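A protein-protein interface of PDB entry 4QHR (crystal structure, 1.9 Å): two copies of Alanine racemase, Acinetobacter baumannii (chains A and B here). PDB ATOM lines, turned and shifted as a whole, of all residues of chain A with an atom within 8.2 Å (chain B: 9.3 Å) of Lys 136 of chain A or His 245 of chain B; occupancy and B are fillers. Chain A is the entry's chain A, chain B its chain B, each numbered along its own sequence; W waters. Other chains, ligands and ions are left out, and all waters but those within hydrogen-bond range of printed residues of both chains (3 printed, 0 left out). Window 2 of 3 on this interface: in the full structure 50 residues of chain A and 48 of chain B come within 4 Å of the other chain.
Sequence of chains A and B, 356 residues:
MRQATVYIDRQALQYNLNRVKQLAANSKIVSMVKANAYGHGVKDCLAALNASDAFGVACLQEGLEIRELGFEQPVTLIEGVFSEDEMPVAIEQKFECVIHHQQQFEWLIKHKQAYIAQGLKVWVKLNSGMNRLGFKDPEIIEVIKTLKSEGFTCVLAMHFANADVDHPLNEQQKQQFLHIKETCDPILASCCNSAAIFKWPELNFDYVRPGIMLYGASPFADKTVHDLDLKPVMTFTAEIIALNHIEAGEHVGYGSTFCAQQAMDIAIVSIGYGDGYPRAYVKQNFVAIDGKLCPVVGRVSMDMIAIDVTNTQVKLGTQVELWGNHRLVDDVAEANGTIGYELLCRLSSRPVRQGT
Of chain B, only His 245 comes within 4 Å of Lys 136 of chain A. Of chain A, only Lys 136 (3.3 Å) comes within 4 Å of His 245 of chain B. No residue of chain A comes within 4 Å of Ile 246 of chain B. Of the printed residues of chain A, Ala 242 of chain B touches Leu 133 (3.9 Å). Printed residues of chain A within 4 Å of Ile 268 of chain B: Asn 131 and Arg 132. Ser 128 of chain A touches none of the printed residues of chain B. The nearest residue of chain A that does not touch His 245 of chain B is Asn 131 of chain A (6.1 Å).
Water W3 lies within hydrogen-bond range of the side-chain amide oxygen of Asn 244 of chain B (2.7 Å), the backbone carbonyl oxygen of Gly 134 of chain A (2.8 Å) and the side-chain amide nitrogen of Asn 127 of chain A (3.2 Å). Water W2 bridges a ring nitrogen (ND1) of His 101 of chain A (2.8 Å) and the backbone NH of Leu 243 of chain B (3.0 Å). Water W1 bridges the backbone carbonyl oxygen of Gly 134 of chain A (3.4 Å) and the side-chain amide oxygen of Asn 244 of chain B (3.5 Å).
Of the 22 printed residues of chain A, 4 touch a printed residue of chain B. Printed residues of chain A that touch a printed residue of chain B: Asn 131, Arg 132, Leu 133 and Lys 136. Hydrophobic or aromatic side chains of chain A within 4 Å of the printed part of chain B: Leu 133. Of the 13 printed residues of chain B, 4 touch a printed residue of chain A. Printed residues of chain B that touch a printed residue of chain A: Ala 242, Asn 244, His 245 and Ile 268. Among the printed residues, 6 pairs touch across the chains. Among the printed residues, no Asp or Glu carboxylate lies within 4 Å of a Lys or Arg side-chain nitrogen of the other chain.
Among the printed residues, merely in contact across the chains: Asn 131 of chain A with Ile 268 of chain B, Arg 132 of chain A with Ile 268 of chain B and Leu 133 of chain A with Ala 242 of chain B.
The backbone carbonyl oxygen (O) of Leu 133 of chain A sits at hydrogen-bond distance from the side-chain amino group (NZ) of Lys 125 of chain A (3.2 Å). The backbone NH (N) of Asn 131 of chain A lies within hydrogen-bond range of the side-chain amide oxygen (OD1) of Asn 127 of chain A (3.0 Å). O of Ala 242 of chain B is in hydrogen-bond range of N of Ile 268 of chain B (2.9 Å). The backbone NH of Ile 266 of chain B is in hydrogen-bond range of the backbone carbonyl oxygen of Asn 244 of chain B (2.8 Å).
No position is printed for both chains. Of the 6 pairs that touch across the chains among the printed residues, none has its exchanged pair printed and touching as well.
The backbone carbonyl oxygen (O) of Asn 131 of chain A sits at hydrogen-bond distance from the side-chain amide nitrogen (ND2) of Asn 244 of chain B, at 3.2 Å. The backbone carbonyl oxygen (O) of Arg 132 of chain A sits at hydrogen-bond distance from the side-chain amide nitrogen (ND2) of Asn 244 of chain B (3.0 Å). NZ of Lys 136 of chain A sits at hydrogen-bond distance from O of His 245 of chain B (3.3 Å).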
ATOM      1  N   HIS A 100     -18.960  -0.520  -1.179  1.00  0.00           N
ATOM      2  CA  HIS A 100     -18.546  -1.748  -0.506  1.00  0.00           C
ATOM      3  C   HIS A 100     -17.880  -1.490   0.866  1.00  0.00           C
ATOM      4  O   HIS A 100     -17.605  -2.436   1.573  1.00  0.00           O
ATOM      5  CB  HIS A 100     -17.651  -2.618  -1.414  1.00  0.00           C
ATOM      6  CG  HIS A 100     -16.372  -1.949  -1.795  1.00  0.00           C
ATOM      7  ND1 HIS A 100     -15.304  -1.850  -0.927  1.00  0.00           N
ATOM      8  CD2 HIS A 100     -16.001  -1.323  -2.940  1.00  0.00           C
ATOM      9  CE1 HIS A 100     -14.324  -1.204  -1.530  1.00  0.00           C
ATOM     10  NE2 HIS A 100     -14.735  -0.838  -2.738  1.00  0.00           N
ATOM     11  N   HIS A 101     -17.640  -0.244   1.246  1.00  0.00           N
ATOM     12  CA  HIS A 101     -17.027   0.024   2.540  1.00  0.00           C
ATOM     13  C   HIS A 101     -17.355   1.432   2.980  1.00  0.00           C
ATOM     14  O   HIS A 101     -17.826   2.276   2.170  1.00  0.00           O
ATOM     15  CB  HIS A 101     -15.504  -0.335   2.542  1.00  0.00           C
ATOM     16  CG  HIS A 101     -14.644   0.532   1.665  1.00  0.00           C
ATOM     17  ND1 HIS A 101     -13.294   0.690   1.888  1.00  0.00           N
ATOM     18  CD2 HIS A 101     -14.932   1.292   0.578  1.00  0.00           C
ATOM     19  CE1 HIS A 101     -12.790   1.499   0.977  1.00  0.00           C
ATOM     20  NE2 HIS A 101     -13.763   1.887   0.180  1.00  0.00           N
ATOM     21  N   LYS A 125     -22.914  -3.683  -1.854  1.00  0.00           N
ATOM     22  CA  LYS A 125     -22.224  -4.963  -2.026  1.00  0.00           C
ATOM     23  C   LYS A 125     -22.109  -5.692  -0.678  1.00  0.00           C
ATOM     24  O   LYS A 125     -21.633  -5.147   0.279  1.00  0.00           O
ATOM     25  CB  LYS A 125     -20.838  -4.704  -2.648  1.00  0.00           C
ATOM     26  CG  LYS A 125     -19.832  -5.875  -2.789  1.00  0.00           C
ATOM     27  CD  LYS A 125     -20.309  -7.046  -3.632  1.00  0.00           C
ATOM     28  CE  LYS A 125     -19.150  -7.851  -4.288  1.00  0.00           C
ATOM     29  NZ  LYS A 125     -18.552  -8.848  -3.369  1.00  0.00           N
ATOM     30  N   LEU A 126     -22.535  -6.944  -0.677  1.00  0.00           N
ATOM     31  CA  LEU A 126     -22.408  -7.844   0.439  1.00  0.00           C
ATOM     32  C   LEU A 126     -21.148  -8.678   0.325  1.00  0.00           C
ATOM     33  O   LEU A 126     -20.852  -9.270  -0.725  1.00  0.00           O
ATOM     34  CB  LEU A 126     -23.577  -8.822   0.420  1.00  0.00           C
ATOM     35  CG  LEU A 126     -23.684  -9.945   1.476  1.00  0.00           C
ATOM     36  CD1 LEU A 126     -23.896  -9.369   2.869  1.00  0.00           C
ATOM     37  CD2 LEU A 126     -24.792 -10.912   1.113  1.00  0.00           C
ATOM     38  N   ASN A 127     -20.430  -8.744   1.428  1.00  0.00           N
ATOM     39  CA  ASN A 127     -19.382  -9.754   1.606  1.00  0.00           C
ATOM     40  C   ASN A 127     -20.043 -10.875   2.391  1.00  0.00           C
ATOM     41  O   ASN A 127     -20.293 -10.736   3.615  1.00  0.00           O
ATOM     42  CB  ASN A 127     -18.223  -9.174   2.393  1.00  0.00           C
ATOM     43  CG  ASN A 127     -17.225 -10.225   2.855  1.00  0.00           C
ATOM     44  OD1 ASN A 127     -17.241 -11.411   2.453  1.00  0.00           O
ATOM     45  ND2 ASN A 127     -16.328  -9.782   3.673  1.00  0.00           N
ATOM     46  N   SER A 128     -20.325 -11.963   1.702  1.00  0.00           N
ATOM     47  CA  SER A 128     -21.015 -13.100   2.305  1.00  0.00           C
ATOM     48  C   SER A 128     -20.077 -14.265   2.550  1.00  0.00           C
ATOM     49  O   SER A 128     -20.546 -15.382   2.839  1.00  0.00           O
ATOM     50  CB  SER A 128     -22.151 -13.555   1.374  1.00  0.00           C
ATOM     51  OG  SER A 128     -21.697 -13.853   0.062  1.00  0.00           O
ATOM     52  N   GLY A 129     -18.757 -14.032   2.410  1.00  0.00           N
ATOM     53  CA  GLY A 129     -17.767 -15.127   2.499  1.00  0.00           C
ATOM     54  C   GLY A 129     -16.544 -15.023   1.598  1.00  0.00           C
ATOM     55  O   GLY A 129     -15.524 -15.601   1.901  1.00  0.00           O
ATOM     56  N   ASN A 131     -14.685 -12.504   1.238  1.00  0.00           N
ATOM     57  CA  ASN A 131     -13.751 -11.630   1.955  1.00  0.00           C
ATOM     58  C   ASN A 131     -12.908 -10.682   1.058  1.00  0.00           C
ATOM     59  O   ASN A 131     -11.879 -10.100   1.519  1.00  0.00           O
ATOM     60  CB  ASN A 131     -12.917 -12.445   2.974  1.00  0.00           C
ATOM     61  CG  ASN A 131     -13.692 -12.715   4.268  1.00  0.00           C
ATOM     62  OD1 ASN A 131     -14.233 -11.786   4.881  1.00  0.00           O
ATOM     63  ND2 ASN A 131     -13.748 -13.983   4.694  1.00  0.00           N
ATOM     64  N   ARG A 132     -13.364 -10.492  -0.192  1.00  0.00           N
ATOM     65  CA  ARG A 132     -12.805  -9.465  -1.061  1.00  0.00           C
ATOM     66  C   ARG A 132     -13.483  -8.149  -0.662  1.00  0.00           C
ATOM     67  O   ARG A 132     -13.066  -7.506   0.309  1.00  0.00           O
ATOM     68  CB  ARG A 132     -12.975  -9.801  -2.548  1.00  0.00           C
ATOM     69  N   LEU A 133     -14.520  -7.742  -1.397  1.00  0.00           N
ATOM     70  CA  LEU A 133     -15.165  -6.444  -1.155  1.00  0.00           C
ATOM     71  C   LEU A 133     -16.519  -6.654  -0.532  1.00  0.00           C
ATOM     72  O   LEU A 133     -17.136  -7.657  -0.790  1.00  0.00           O
ATOM     73  CB  LEU A 133     -15.364  -5.687  -2.463  1.00  0.00           C
ATOM     74  CG  LEU A 133     -14.104  -5.316  -3.246  1.00  0.00           C
ATOM     75  CD1 LEU A 133     -14.529  -4.458  -4.418  1.00  0.00           C
ATOM     76  CD2 LEU A 133     -13.051  -4.574  -2.416  1.00  0.00           C
ATOM     77  N   GLY A 134     -16.965  -5.709   0.278  1.00  0.00           N
ATOM     78  CA  GLY A 134     -18.363  -5.674   0.693  1.00  0.00           C
ATOM     79  C   GLY A 134     -18.581  -5.446   2.181  1.00  0.00           C
ATOM     80  O   GLY A 134     -17.654  -5.548   2.975  1.00  0.00           O
ATOM     81  N   PHE A 135     -19.821  -5.097   2.514  1.00  0.00           N
ATOM     82  CA  PHE A 135     -20.250  -4.984   3.902  1.00  0.00           C
ATOM     83  C   PHE A 135     -20.647  -6.347   4.397  1.00  0.00           C
ATOM     84  O   PHE A 135     -21.215  -7.118   3.670  1.00  0.00           O
ATOM     85  CB  PHE A 135     -21.427  -4.059   4.048  1.00  0.00           C
ATOM     86  CG  PHE A 135     -21.106  -2.648   3.707  1.00  0.00           C
ATOM     87  CD1 PHE A 135     -20.494  -1.804   4.643  1.00  0.00           C
ATOM     88  CD2 PHE A 135     -21.397  -2.143   2.433  1.00  0.00           C
ATOM     89  CE1 PHE A 135     -20.195  -0.498   4.325  1.00  0.00           C
ATOM     90  CE2 PHE A 135     -21.085  -0.824   2.125  1.00  0.00           C
ATOM     91  CZ  PHE A 135     -20.478  -0.006   3.073  1.00  0.00           C
ATOM     92  N   LYS A 136     -20.345  -6.624   5.646  1.00  0.00           N
ATOM     93  CA  LYS A 136     -20.721  -7.901   6.251  1.00  0.00           C
ATOM     94  C   LYS A 136     -22.138  -7.836   6.834  1.00  0.00           C
ATOM     95  O   LYS A 136     -22.718  -6.764   6.982  1.00  0.00           O
ATOM     96  CB  LYS A 136     -19.714  -8.254   7.359  1.00  0.00           C
ATOM     97  CG  LYS A 136     -18.363  -8.645   6.813  1.00  0.00           C
ATOM     98  CD  LYS A 136     -17.191  -8.490   7.779  1.00  0.00           C
ATOM     99  CE  LYS A 136     -15.923  -9.079   7.167  1.00  0.00           C
ATOM    100  NZ  LYS A 136     -14.761  -9.168   8.101  1.00  0.00           N
ATOM    101  N   ASP A 137     -22.682  -8.999   7.145  1.00  0.00           N
ATOM    102  CA  ASP A 137     -23.943  -9.120   7.859  1.00  0.00           C
ATOM    103  C   ASP A 137     -23.530  -9.101   9.324  1.00  0.00           C
ATOM    104  O   ASP A 137     -22.760  -9.984   9.685  1.00  0.00           O
ATOM    105  CB  ASP A 137     -24.601 -10.448   7.487  1.00  0.00           C
ATOM    106  CG  ASP A 137     -25.888 -10.705   8.256  1.00  0.00           C
ATOM    107  OD1 ASP A 137     -26.289  -9.864   9.077  1.00  0.00           O
ATOM    108  OD2 ASP A 137     -26.507 -11.750   8.004  1.00  0.00           O
ATOM    109  N   PRO A 138     -24.037  -8.199  10.174  1.00  0.00           N
ATOM    110  CA  PRO A 138     -25.271  -7.389   9.923  1.00  0.00           C
ATOM    111  C   PRO A 138     -25.116  -5.943   9.520  1.00  0.00           C
ATOM    112  O   PRO A 138     -26.136  -5.316   9.249  1.00  0.00           O
ATOM    113  CB  PRO A 138     -25.988  -7.433  11.298  1.00  0.00           C
ATOM    114  CG  PRO A 138     -24.862  -7.496  12.285  1.00  0.00           C
ATOM    115  CD  PRO A 138     -23.788  -8.355  11.634  1.00  0.00           C
ATOM    116  N   GLU A 139     -23.891  -5.424   9.450  1.00  0.00           N
ATOM    117  CA  GLU A 139     -23.646  -4.028   9.099  1.00  0.00           C
ATOM    118  C   GLU A 139     -24.315  -3.542   7.833  1.00  0.00           C
ATOM    119  O   GLU A 139     -24.723  -2.398   7.761  1.00  0.00           O
ATOM    120  CB  GLU A 139     -22.165  -3.766   8.901  1.00  0.00           C
ATOM    121  N   ILE A 140     -24.397  -4.408   6.836  1.00  0.00           N
ATOM    122  CA  ILE A 140     -25.030  -4.093   5.561  1.00  0.00           C
ATOM    123  C   ILE A 140     -26.497  -3.698   5.724  1.00  0.00           C
ATOM    124  O   ILE A 140     -27.009  -2.889   4.973  1.00  0.00           O
ATOM    125  CB  ILE A 140     -24.874  -5.233   4.525  1.00  0.00           C
ATOM    126  CG1 ILE A 140     -25.161  -4.695   3.116  1.00  0.00           C
ATOM    127  CG2 ILE A 140     -25.794  -6.400   4.787  1.00  0.00           C
ATOM    128  CD1 ILE A 140     -24.760  -5.612   1.974  1.00  0.00           C
ATOM    129  N   ILE A 141     -27.164  -4.247   6.731  1.00  0.00           N
ATOM    130  CA  ILE A 141     -28.585  -3.941   6.953  1.00  0.00           C
ATOM    131  C   ILE A 141     -28.738  -2.503   7.390  1.00  0.00           C
ATOM    132  O   ILE A 141     -29.613  -1.809   6.906  1.00  0.00           O
ATOM    133  CB  ILE A 141     -29.239  -4.911   7.955  1.00  0.00           C
ATOM    134  CG1 ILE A 141     -29.196  -6.316   7.387  1.00  0.00           C
ATOM    135  CG2 ILE A 141     -30.687  -4.482   8.267  1.00  0.00           C
ATOM    136  CD1 ILE A 141     -29.451  -7.396   8.415  1.00  0.00           C
ATOM    137  N   GLU A 142     -27.852  -2.027   8.244  1.00  0.00           N
ATOM    138  CA  GLU A 142     -27.941  -0.659   8.702  1.00  0.00           C
ATOM    139  C   GLU A 142     -27.612   0.297   7.596  1.00  0.00           C
ATOM    140  O   GLU A 142     -28.235   1.337   7.509  1.00  0.00           O
ATOM    141  CB  GLU A 142     -27.041  -0.444   9.927  1.00  0.00           C
ATOM    142  CG  GLU A 142     -27.397  -1.436  11.051  1.00  0.00           C
ATOM    143  CD  GLU A 142     -28.889  -1.366  11.395  1.00  0.00           C
ATOM    144  OE1 GLU A 142     -29.301  -0.238  11.786  1.00  0.00           O
ATOM    145  OE2 GLU A 142     -29.646  -2.383  11.271  1.00  0.00           O
ATOM    146  N   VAL A 143     -26.631  -0.069   6.756  1.00  0.00           N
ATOM    147  CA  VAL A 143     -26.234   0.744   5.603  1.00  0.00           C
ATOM    148  C   VAL A 143     -27.447   0.896   4.703  1.00  0.00           C
ATOM    149  O   VAL A 143     -27.819   1.970   4.371  1.00  0.00           O
ATOM    150  CB  VAL A 143     -25.057   0.104   4.832  1.00  0.00           C
ATOM    151  CG1 VAL A 143     -24.813   0.786   3.487  1.00  0.00           C
ATOM    152  CG2 VAL A 143     -23.788   0.149   5.677  1.00  0.00           C
ATOM    153  N   GLN A 176     -27.094 -16.554   2.950  1.00  0.00           N
ATOM    154  CA  GLN A 176     -26.749 -15.225   3.437  1.00  0.00           C
ATOM    155  C   GLN A 176     -27.465 -14.130   2.578  1.00  0.00           C
ATOM    156  O   GLN A 176     -28.101 -13.202   3.111  1.00  0.00           O
ATOM    157  CB  GLN A 176     -25.234 -15.071   3.450  1.00  0.00           C
ATOM    158  CG  GLN A 176     -24.737 -13.765   4.001  1.00  0.00           C
ATOM    159  CD  GLN A 176     -23.480 -13.924   4.830  1.00  0.00           C
ATOM    160  OE1 GLN A 176     -22.917 -15.012   4.917  1.00  0.00           O
ATOM    161  NE2 GLN A 176     -23.027 -12.833   5.440  1.00  0.00           N
ATOM    162  N   ILE A 180     -30.562 -11.514   3.732  1.00  0.00           N
ATOM    163  CA  ILE A 180     -30.440 -10.081   3.681  1.00  0.00           C
ATOM    164  C   ILE A 180     -31.543  -9.519   2.811  1.00  0.00           C
ATOM    165  O   ILE A 180     -32.124  -8.517   3.161  1.00  0.00           O
ATOM    166  CB  ILE A 180     -29.046  -9.620   3.220  1.00  0.00           C
ATOM    167  CG1 ILE A 180     -27.963 -10.097   4.202  1.00  0.00           C
ATOM    168  CG2 ILE A 180     -29.013  -8.099   3.155  1.00  0.00           C
ATOM    169  CD1 ILE A 180     -27.993  -9.428   5.570  1.00  0.00           C
ATOM    170  N   ALA B 242      -9.257  -1.631  -0.012  1.00  0.00           N
ATOM    171  CA  ALA B 242     -10.097  -2.013   1.106  1.00  0.00           C
ATOM    172  C   ALA B 242      -9.231  -2.738   2.147  1.00  0.00           C
ATOM    173  O   ALA B 242      -8.244  -3.355   1.807  1.00  0.00           O
ATOM    174  CB  ALA B 242     -11.229  -2.950   0.622  1.00  0.00           C
ATOM    175  N   LEU B 243      -9.631  -2.665   3.410  1.00  0.00           N
ATOM    176  CA  LEU B 243      -8.978  -3.380   4.482  1.00  0.00           C
ATOM    177  C   LEU B 243      -9.996  -4.172   5.246  1.00  0.00           C
ATOM    178  O   LEU B 243     -11.048  -3.628   5.594  1.00  0.00           O
ATOM    179  CB  LEU B 243      -8.290  -2.373   5.434  1.00  0.00           C
ATOM    180  CG  LEU B 243      -7.106  -1.619   4.847  1.00  0.00           C
ATOM    181  CD1 LEU B 243      -6.636  -0.428   5.666  1.00  0.00           C
ATOM    182  CD2 LEU B 243      -5.947  -2.580   4.683  1.00  0.00           C
ATOM    183  N   ASN B 244      -9.682  -5.449   5.514  1.00  0.00           N
ATOM    184  CA  ASN B 244     -10.579  -6.329   6.293  1.00  0.00           C
ATOM    185  C   ASN B 244      -9.837  -7.023   7.402  1.00  0.00           C
ATOM    186  O   ASN B 244      -8.758  -7.475   7.175  1.00  0.00           O
ATOM    187  CB  ASN B 244     -11.197  -7.421   5.424  1.00  0.00           C
ATOM    188  CG  ASN B 244     -12.045  -6.853   4.324  1.00  0.00           C
ATOM    189  OD1 ASN B 244     -12.856  -5.960   4.572  1.00  0.00           O
ATOM    190  ND2 ASN B 244     -11.859  -7.345   3.084  1.00  0.00           N
ATOM    191  N   HIS B 245     -10.438  -7.100   8.592  1.00  0.00           N
ATOM    192  CA  HIS B 245      -9.923  -7.900   9.748  1.00  0.00           C
ATOM    193  C   HIS B 245     -10.683  -9.205   9.720  1.00  0.00           C
ATOM    194  O   HIS B 245     -11.892  -9.139   9.817  1.00  0.00           O
ATOM    195  CB  HIS B 245     -10.237  -7.174  11.061  1.00  0.00           C
ATOM    196  N   ILE B 246     -10.028 -10.364   9.570  1.00  0.00           N
ATOM    197  CA  ILE B 246     -10.728 -11.660   9.392  1.00  0.00           C
ATOM    198  C   ILE B 246     -10.448 -12.580  10.574  1.00  0.00           C
ATOM    199  O   ILE B 246      -9.274 -12.850  10.820  1.00  0.00           O
ATOM    200  CB  ILE B 246     -10.287 -12.428   8.131  1.00  0.00           C
ATOM    201  N   MET B 264      -6.200 -12.450  10.918  1.00  0.00           N
ATOM    202  CA  MET B 264      -5.448 -11.655   9.950  1.00  0.00           C
ATOM    203  C   MET B 264      -6.070 -10.300   9.536  1.00  0.00           C
ATOM    204  O   MET B 264      -7.296 -10.065   9.631  1.00  0.00           O
ATOM    205  CB  MET B 264      -5.255 -12.449   8.659  1.00  0.00           C
ATOM    206  CG  MET B 264      -4.753 -13.881   8.792  1.00  0.00           C
ATOM    207  SD  MET B 264      -4.992 -14.704   7.204  1.00  0.00           S
ATOM    208  CE  MET B 264      -3.935 -13.806   6.068  1.00  0.00           C
ATOM    209  N   ASP B 265      -5.203  -9.413   9.056  1.00  0.00           N
ATOM    210  CA  ASP B 265      -5.621  -8.197   8.406  1.00  0.00           C
ATOM    211  C   ASP B 265      -5.325  -8.413   6.927  1.00  0.00           C
ATOM    212  O   ASP B 265      -4.248  -8.847   6.603  1.00  0.00           O
ATOM    213  CB  ASP B 265      -4.839  -7.017   8.903  1.00  0.00           C
ATOM    214  CG  ASP B 265      -5.105  -6.724  10.365  1.00  0.00           C
ATOM    215  OD1 ASP B 265      -6.268  -6.636  10.754  1.00  0.00           O
ATOM    216  OD2 ASP B 265      -4.121  -6.588  11.110  1.00  0.00           O
ATOM    217  N   ILE B 266      -6.291  -8.104   6.066  1.00  0.00           N
ATOM    218  CA  ILE B 266      -6.216  -8.411   4.667  1.00  0.00           C
ATOM    219  C   ILE B 266      -6.373  -7.078   3.959  1.00  0.00           C
ATOM    220  O   ILE B 266      -7.236  -6.313   4.345  1.00  0.00           O
ATOM    221  CB  ILE B 266      -7.426  -9.315   4.226  1.00  0.00           C
ATOM    222  CG1 ILE B 266      -7.362 -10.701   4.866  1.00  0.00           C
ATOM    223  CG2 ILE B 266      -7.525  -9.482   2.729  1.00  0.00           C
ATOM    224  CD1 ILE B 266      -6.061 -11.456   4.730  1.00  0.00           C
ATOM    225  N   ALA B 267      -5.590  -6.838   2.908  1.00  0.00           N
ATOM    226  CA  ALA B 267      -5.768  -5.655   2.117  1.00  0.00           C
ATOM    227  C   ALA B 267      -6.109  -6.116   0.707  1.00  0.00           C
ATOM    228  O   ALA B 267      -5.521  -7.079   0.178  1.00  0.00           O
ATOM    229  CB  ALA B 267      -4.514  -4.823   2.131  1.00  0.00           C
ATOM    230  N   ILE B 268      -7.085  -5.440   0.110  1.00  0.00           N
ATOM    231  CA  ILE B 268      -7.436  -5.683  -1.258  1.00  0.00           C
ATOM    232  C   ILE B 268      -6.728  -4.597  -2.083  1.00  0.00           C
ATOM    233  O   ILE B 268      -6.701  -3.429  -1.711  1.00  0.00           O
ATOM    234  CB  ILE B 268      -8.962  -5.642  -1.496  1.00  0.00           C
ATOM    235  CG1 ILE B 268      -9.706  -6.565  -0.515  1.00  0.00           C
ATOM    236  CG2 ILE B 268      -9.264  -5.960  -2.964  1.00  0.00           C
ATOM    237  CD1 ILE B 268      -9.136  -7.952  -0.426  1.00  0.00           C
ATOM    238  N   ILE B 307      -3.943  -9.384  -0.133  1.00  0.00           N
ATOM    239  CA  ILE B 307      -2.627  -9.525   0.481  1.00  0.00           C
ATOM    240  C   ILE B 307      -2.749  -9.556   2.017  1.00  0.00           C
ATOM    241  O   ILE B 307      -3.613  -8.922   2.589  1.00  0.00           O
ATOM    242  CB  ILE B 307      -1.625  -8.460   0.009  1.00  0.00           C
ATOM    243  CG1 ILE B 307      -2.039  -7.109   0.466  1.00  0.00           C
ATOM    244  CG2 ILE B 307      -1.486  -8.416  -1.539  1.00  0.00           C
ATOM    245  CD1 ILE B 307      -0.869  -6.136   0.512  1.00  0.00           C
ATOM    246  N   VAL B 309      -1.552  -8.324   5.356  1.00  0.00           N
ATOM    247  CA  VAL B 309      -0.865  -7.166   5.932  1.00  0.00           C
ATOM    248  C   VAL B 309      -0.881  -7.239   7.457  1.00  0.00           C
ATOM    249  O   VAL B 309      -0.674  -6.218   8.154  1.00  0.00           O
ATOM    250  CB  VAL B 309      -1.438  -5.798   5.431  1.00  0.00           C
ATOM    251  CG1 VAL B 309      -1.142  -5.607   3.934  1.00  0.00           C
ATOM    252  CG2 VAL B 309      -2.937  -5.654   5.646  1.00  0.00           C
ATOM    253  N   THR B 310      -1.122  -8.429   7.996  1.00  0.00           N
ATOM    254  CA  THR B 310      -1.133  -8.607   9.435  1.00  0.00           C
ATOM    255  C   THR B 310       0.142  -7.979  10.071  1.00  0.00           C
ATOM    256  O   THR B 310       0.108  -7.324  11.114  1.00  0.00           O
ATOM    257  CB  THR B 310      -1.281 -10.106   9.836  1.00  0.00           C
ATOM    258  OG1 THR B 310      -2.390 -10.721   9.140  1.00  0.00           O
ATOM    259  CG2 THR B 310      -1.534 -10.237  11.384  1.00  0.00           C
HETATM  260  O   HOH W   1     -15.964  -5.196   5.909  1.00  0.00           O
HETATM  261  O   HOH W   2     -12.153  -1.101   3.785  1.00  0.00           O
HETATM  262  O   HOH W   3     -15.183  -6.805   3.391  1.00  0.00           O
